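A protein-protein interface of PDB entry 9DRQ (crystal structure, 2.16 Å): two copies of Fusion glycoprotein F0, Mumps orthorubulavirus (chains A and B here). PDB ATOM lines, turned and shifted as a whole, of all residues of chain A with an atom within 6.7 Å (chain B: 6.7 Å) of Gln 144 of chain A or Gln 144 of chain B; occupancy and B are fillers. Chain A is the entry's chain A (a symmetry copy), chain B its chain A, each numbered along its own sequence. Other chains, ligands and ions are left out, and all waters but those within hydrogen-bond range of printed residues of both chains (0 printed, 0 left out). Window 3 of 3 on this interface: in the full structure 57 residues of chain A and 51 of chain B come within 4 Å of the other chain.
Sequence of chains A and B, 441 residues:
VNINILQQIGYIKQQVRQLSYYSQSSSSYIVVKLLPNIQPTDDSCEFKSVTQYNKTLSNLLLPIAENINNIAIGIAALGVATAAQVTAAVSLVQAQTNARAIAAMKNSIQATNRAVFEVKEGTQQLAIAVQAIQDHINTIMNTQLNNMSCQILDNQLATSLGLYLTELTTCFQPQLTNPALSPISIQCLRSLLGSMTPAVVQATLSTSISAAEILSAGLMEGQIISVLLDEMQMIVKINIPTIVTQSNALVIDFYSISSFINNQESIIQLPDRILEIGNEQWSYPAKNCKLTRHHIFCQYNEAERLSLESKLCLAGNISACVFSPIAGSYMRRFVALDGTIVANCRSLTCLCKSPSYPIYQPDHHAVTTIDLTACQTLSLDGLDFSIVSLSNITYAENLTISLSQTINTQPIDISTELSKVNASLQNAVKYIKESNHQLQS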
ATOM      1  N   THR A 139       6.024 -31.392 -19.005  1.00  0.00           N
ATOM      2  CA  THR A 139       5.527 -30.226 -19.719  1.00  0.00           C
ATOM      3  C   THR A 139       6.659 -29.501 -20.423  1.00  0.00           C
ATOM      4  O   THR A 139       6.526 -29.138 -21.589  1.00  0.00           O
ATOM      5  CB  THR A 139       4.785 -29.281 -18.789  1.00  0.00           C
ATOM      6  OG1 THR A 139       3.756 -30.006 -18.111  1.00  0.00           O
ATOM      7  CG2 THR A 139       4.128 -28.179 -19.600  1.00  0.00           C
ATOM      8  N   ILE A 140       7.800 -29.333 -19.758  1.00  0.00           N
ATOM      9  CA  ILE A 140       8.935 -28.695 -20.416  1.00  0.00           C
ATOM     10  C   ILE A 140       9.305 -29.446 -21.691  1.00  0.00           C
ATOM     11  O   ILE A 140       9.527 -28.839 -22.743  1.00  0.00           O
ATOM     12  CB  ILE A 140      10.145 -28.607 -19.465  1.00  0.00           C
ATOM     13  CG1 ILE A 140       9.821 -27.788 -18.206  1.00  0.00           C
ATOM     14  CG2 ILE A 140      11.383 -28.083 -20.214  1.00  0.00           C
ATOM     15  CD1 ILE A 140       8.873 -26.625 -18.427  1.00  0.00           C
ATOM     16  N   ASN A 142       7.671 -31.180 -23.787  1.00  0.00           N
ATOM     17  CA  ASN A 142       6.895 -31.246 -25.018  1.00  0.00           C
ATOM     18  C   ASN A 142       6.112 -29.965 -25.301  1.00  0.00           C
ATOM     19  O   ASN A 142       5.115 -29.997 -26.029  1.00  0.00           O
ATOM     20  CB  ASN A 142       5.981 -32.487 -25.041  1.00  0.00           C
ATOM     21  CG  ASN A 142       4.717 -32.319 -24.244  1.00  0.00           C
ATOM     22  OD1 ASN A 142       4.754 -31.888 -23.095  1.00  0.00           O
ATOM     23  ND2 ASN A 142       3.580 -32.668 -24.851  1.00  0.00           N
ATOM     24  N   THR A 143       6.564 -28.819 -24.797  1.00  0.00           N
ATOM     25  CA  THR A 143       6.023 -27.565 -25.305  1.00  0.00           C
ATOM     26  C   THR A 143       6.769 -27.188 -26.572  1.00  0.00           C
ATOM     27  O   THR A 143       8.001 -27.287 -26.636  1.00  0.00           O
ATOM     28  CB  THR A 143       6.131 -26.422 -24.299  1.00  0.00           C
ATOM     29  OG1 THR A 143       7.493 -26.007 -24.207  1.00  0.00           O
ATOM     30  CG2 THR A 143       5.649 -26.862 -22.973  1.00  0.00           C
ATOM     31  N   GLN A 144       6.014 -26.774 -27.578  1.00  0.00           N
ATOM     32  CA  GLN A 144       6.590 -26.233 -28.798  1.00  0.00           C
ATOM     33  C   GLN A 144       7.233 -24.888 -28.503  1.00  0.00           C
ATOM     34  O   GLN A 144       6.606 -24.013 -27.901  1.00  0.00           O
ATOM     35  CB  GLN A 144       5.505 -26.078 -29.858  1.00  0.00           C
ATOM     36  CG  GLN A 144       4.878 -27.390 -30.292  1.00  0.00           C
ATOM     37  CD  GLN A 144       3.954 -27.248 -31.502  1.00  0.00           C
ATOM     38  OE1 GLN A 144       4.045 -26.287 -32.275  1.00  0.00           O
ATOM     39  NE2 GLN A 144       3.058 -28.210 -31.661  1.00  0.00           N
ATOM     40  N   LEU A 145       8.483 -24.729 -28.913  1.00  0.00           N
ATOM     41  CA  LEU A 145       9.194 -23.467 -28.792  1.00  0.00           C
ATOM     42  C   LEU A 145       9.408 -22.840 -30.170  1.00  0.00           C
ATOM     43  O   LEU A 145       9.439 -23.538 -31.191  1.00  0.00           O
ATOM     44  CB  LEU A 145      10.535 -23.681 -28.078  1.00  0.00           C
ATOM     45  CG  LEU A 145      10.443 -24.286 -26.661  1.00  0.00           C
ATOM     46  CD1 LEU A 145      11.813 -24.671 -26.109  1.00  0.00           C
ATOM     47  CD2 LEU A 145       9.704 -23.363 -25.669  1.00  0.00           C
ATOM     48  N   ASN A 146       9.547 -21.508 -30.199  1.00  0.00           N
ATOM     49  CA  ASN A 146      10.052 -20.859 -31.409  1.00  0.00           C
ATOM     50  C   ASN A 146      11.426 -21.394 -31.767  1.00  0.00           C
ATOM     51  O   ASN A 146      11.748 -21.611 -32.940  1.00  0.00           O
ATOM     52  CB  ASN A 146      10.126 -19.347 -31.220  1.00  0.00           C
ATOM     53  CG  ASN A 146       8.773 -18.721 -31.051  1.00  0.00           C
ATOM     54  OD1 ASN A 146       7.768 -19.264 -31.498  1.00  0.00           O
ATOM     55  ND2 ASN A 146       8.734 -17.569 -30.398  1.00  0.00           N
ATOM     56  N   ASN A 147      12.225 -21.658 -30.758  1.00  0.00           N
ATOM     57  CA  ASN A 147      13.616 -22.041 -30.899  1.00  0.00           C
ATOM     58  C   ASN A 147      13.836 -23.226 -29.969  1.00  0.00           C
ATOM     59  O   ASN A 147      13.955 -23.054 -28.752  1.00  0.00           O
ATOM     60  CB  ASN A 147      14.469 -20.865 -30.518  1.00  0.00           C
ATOM     61  CG  ASN A 147      15.880 -21.019 -30.901  1.00  0.00           C
ATOM     62  OD1 ASN A 147      16.410 -22.108 -31.125  1.00  0.00           O
ATOM     63  ND2 ASN A 147      16.509 -19.884 -30.978  1.00  0.00           N
ATOM     64  N   MET A 148      13.834 -24.423 -30.534  1.00  0.00           N
ATOM     65  CA  MET A 148      14.036 -25.645 -29.773  1.00  0.00           C
ATOM     66  C   MET A 148      15.491 -26.056 -29.946  1.00  0.00           C
ATOM     67  O   MET A 148      15.894 -26.476 -31.037  1.00  0.00           O
ATOM     68  CB  MET A 148      13.092 -26.746 -30.241  1.00  0.00           C
ATOM     69  CG  MET A 148      13.215 -28.012 -29.435  1.00  0.00           C
ATOM     70  SD  MET A 148      12.717 -27.697 -27.746  1.00  0.00           S
ATOM     71  CE  MET A 148      10.939 -27.614 -27.949  1.00  0.00           C
ATOM     72  N   THR B 139      11.853 -18.702 -21.250  1.00  0.00           N
ATOM     73  CA  THR B 139      10.904 -19.728 -21.655  1.00  0.00           C
ATOM     74  C   THR B 139       9.558 -19.115 -21.995  1.00  0.00           C
ATOM     75  O   THR B 139       8.967 -19.454 -23.017  1.00  0.00           O
ATOM     76  CB  THR B 139      10.749 -20.795 -20.584  1.00  0.00           C
ATOM     77  OG1 THR B 139      12.040 -21.319 -20.258  1.00  0.00           O
ATOM     78  CG2 THR B 139       9.901 -21.934 -21.118  1.00  0.00           C
ATOM     79  N   ILE B 140       9.082 -18.170 -21.186  1.00  0.00           N
ATOM     80  CA  ILE B 140       7.819 -17.511 -21.506  1.00  0.00           C
ATOM     81  C   ILE B 140       7.884 -16.879 -22.891  1.00  0.00           C
ATOM     82  O   ILE B 140       6.959 -17.020 -23.697  1.00  0.00           O
ATOM     83  CB  ILE B 140       7.464 -16.456 -20.440  1.00  0.00           C
ATOM     84  CG1 ILE B 140       7.318 -17.083 -19.045  1.00  0.00           C
ATOM     85  CG2 ILE B 140       6.221 -15.655 -20.868  1.00  0.00           C
ATOM     86  CD1 ILE B 140       6.733 -18.481 -19.032  1.00  0.00           C
ATOM     87  N   ASN B 142       9.459 -17.558 -25.562  1.00  0.00           N
ATOM     88  CA  ASN B 142       9.508 -18.257 -26.839  1.00  0.00           C
ATOM     89  C   ASN B 142       8.729 -19.570 -26.833  1.00  0.00           C
ATOM     90  O   ASN B 142       9.005 -20.457 -27.647  1.00  0.00           O
ATOM     91  CB  ASN B 142      10.960 -18.459 -27.315  1.00  0.00           C
ATOM     92  CG  ASN B 142      11.655 -19.614 -26.648  1.00  0.00           C
ATOM     93  OD1 ASN B 142      11.628 -19.742 -25.428  1.00  0.00           O
ATOM     94  ND2 ASN B 142      12.297 -20.466 -27.452  1.00  0.00           N
ATOM     95  N   THR B 143       7.718 -19.707 -25.979  1.00  0.00           N
ATOM     96  CA  THR B 143       6.779 -20.805 -26.167  1.00  0.00           C
ATOM     97  C   THR B 143       5.733 -20.386 -27.184  1.00  0.00           C
ATOM     98  O   THR B 143       5.216 -19.262 -27.136  1.00  0.00           O
ATOM     99  CB  THR B 143       6.084 -21.220 -24.873  1.00  0.00           C
ATOM    100  OG1 THR B 143       5.127 -20.225 -24.516  1.00  0.00           O
ATOM    101  CG2 THR B 143       7.075 -21.376 -23.789  1.00  0.00           C
ATOM    102  N   GLN B 144       5.443 -21.288 -28.109  1.00  0.00           N
ATOM    103  CA  GLN B 144       4.354 -21.095 -29.054  1.00  0.00           C
ATOM    104  C   GLN B 144       3.025 -21.168 -28.320  1.00  0.00           C
ATOM    105  O   GLN B 144       2.777 -22.114 -27.569  1.00  0.00           O
ATOM    106  CB  GLN B 144       4.417 -22.162 -30.141  1.00  0.00           C
ATOM    107  CG  GLN B 144       5.669 -22.097 -30.996  1.00  0.00           C
ATOM    108  CD  GLN B 144       5.621 -23.023 -32.211  1.00  0.00           C
ATOM    109  OE1 GLN B 144       4.549 -23.439 -32.664  1.00  0.00           O
ATOM    110  NE2 GLN B 144       6.792 -23.351 -32.735  1.00  0.00           N
ATOM    111  N   LEU B 145       2.181 -20.167 -28.526  1.00  0.00           N
ATOM    112  CA  LEU B 145       0.837 -20.148 -27.975  1.00  0.00           C
ATOM    113  C   LEU B 145      -0.198 -20.319 -29.086  1.00  0.00           C
ATOM    114  O   LEU B 145       0.057 -19.997 -30.252  1.00  0.00           O
ATOM    115  CB  LEU B 145       0.599 -18.842 -27.206  1.00  0.00           C
ATOM    116  CG  LEU B 145       1.570 -18.572 -26.037  1.00  0.00           C
ATOM    117  CD1 LEU B 145       1.413 -17.165 -25.469  1.00  0.00           C
ATOM    118  CD2 LEU B 145       1.453 -19.624 -24.914  1.00  0.00           C
ATOM    119  N   ASN B 146      -1.377 -20.841 -28.721  1.00  0.00           N
ATOM    120  CA  ASN B 146      -2.518 -20.762 -29.633  1.00  0.00           C
ATOM    121  C   ASN B 146      -2.829 -19.315 -29.973  1.00  0.00           C
ATOM    122  O   ASN B 146      -3.155 -18.978 -31.116  1.00  0.00           O
ATOM    123  CB  ASN B 146      -3.749 -21.417 -29.016  1.00  0.00           C
ATOM    124  CG  ASN B 146      -3.581 -22.896 -28.829  1.00  0.00           C
ATOM    125  OD1 ASN B 146      -2.793 -23.532 -29.521  1.00  0.00           O
ATOM    126  ND2 ASN B 146      -4.321 -23.458 -27.885  1.00  0.00           N
ATOM    127  N   ASN B 147      -2.682 -18.447 -28.998  1.00  0.00           N
ATOM    128  CA  ASN B 147      -3.061 -17.051 -29.085  1.00  0.00           C
ATOM    129  C   ASN B 147      -1.903 -16.249 -28.510  1.00  0.00           C
ATOM    130  O   ASN B 147      -1.734 -16.178 -27.289  1.00  0.00           O
ATOM    131  CB  ASN B 147      -4.324 -16.856 -28.295  1.00  0.00           C
ATOM    132  CG  ASN B 147      -4.975 -15.562 -28.546  1.00  0.00           C
ATOM    133  OD1 ASN B 147      -4.390 -14.582 -29.009  1.00  0.00           O
ATOM    134  ND2 ASN B 147      -6.236 -15.561 -28.227  1.00  0.00           N
ATOM    135  N   MET B 148      -1.079 -15.698 -29.388  1.00  0.00           N
ATOM    136  CA  MET B 148       0.069 -14.900 -28.987  1.00  0.00           C
ATOM    137  C   MET B 148      -0.328 -13.436 -29.106  1.00  0.00           C
ATOM    138  O   MET B 148      -0.499 -12.926 -30.220  1.00  0.00           O
ATOM    139  CB  MET B 148       1.285 -15.216 -29.850  1.00  0.00           C
ATOM    140  CG  MET B 148       2.519 -14.464 -29.427  1.00  0.00           C
ATOM    141  SD  MET B 148       3.002 -14.983 -27.785  1.00  0.00           S
ATOM    142  CE  MET B 148       3.709 -16.588 -28.152  1.00  0.00           C
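Thr 143 of chain B touches Gln 144 of chain A.
Asn 142 of chain B touches Leu 145 of chain A.
Leu 145 of chain A touches Thr 143 of chain B (CD2 to CG2, 3.8 Å).
Asn 146 of chain A touches Gln 144 of chain B.
Asn 142 of chain A touches none of the printed residues of chain B.
Of chain B, only Thr 143 and Gln 144 come within 4 Å of Gln 144 of chain A.
Of the printed residues of chain B, Leu 145 of chain A touches Asn 142 (3.2 Å), Thr 143 (3.8 Å) and Gln 144 (3.1 Å).
Of the printed residues of chain B, Asn 146 of chain A touches Asn 142 (2.8 Å) and Gln 144 (3.6 Å).
Of the printed residues of chain B, Asn 147 of chain A touches Asn 142.
Of the printed residues of chain A, Asn 142 of chain B touches Leu 145, Asn 146 and Asn 147.
Of the printed residues of chain A, Thr 143 of chain B touches Gln 144 (3.7 Å) and Leu 145 (3.8 Å).
Of chain A, only Gln 144 (2.9 Å), Leu 145 (3.1 Å) and Asn 146 (3.6 Å) come within 4 Å of Gln 144 of chain B.
Asn 146 of chain B touches none of the printed residues of chain A.
The nearest residue of chain B that does not touch Gln 144 of chain A is Asn 142 of chain B (4.3 Å).
The side-chain amide nitrogen of Gln 144 of chain B is in hydrogen-bond range of the backbone carbonyl oxygen of Leu 145 of chain A, at 3.1 Å.
The backbone NH (N) of Asn 146 of chain A lies within hydrogen-bond range of the backbone carbonyl oxygen (O) of Asn 142 of chain B (2.8 Å).
OE1 of Gln 144 of chain B lies close to OE1 of Gln 144 of chain A, 2.9 Å away.
The side-chain amide nitrogen (ND2) of Asn 142 of chain B lies within hydrogen-bond range of the backbone carbonyl oxygen (O) of Asn 147 of chain A, at 3.3 Å.
Leu 145 of chain A touches Asn 142 of chain B, but with the chains exchanged Asn 142 of chain A does not touch Leu 145 of chain B (10.6 Å).
Leu 145 of chain A touches Gln 144 of chain B, but with the chains exchanged Gln 144 of chain A does not touch Leu 145 of chain B (5.9 Å).
Asn 146 of chain A touches Asn 142 of chain B, but with the chains exchanged Asn 142 of chain A does not touch Asn 146 of chain B (10.8 Å).
Asn 146 of chain A touches Gln 144 of chain B, but with the chains exchanged Gln 144 of chain A does not touch Asn 146 of chain B (7.8 Å).
Positions printed for both chains: 139, 140, 142, 143, 144, 145, 146, 147 and 148.
Of the 8 pairs that touch across the chains among the printed residues, 1 has its exchanged pair printed and touching as well.
Of the 9 printed residues of chain A, 4 touch a printed residue of chain B.
Among the printed residues, 8 pairs touch across the chains.
Among the printed residues, no Asp or Glu carboxylate lies within 4 Å of a Lys or Arg side-chain nitrogen of the other chain.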
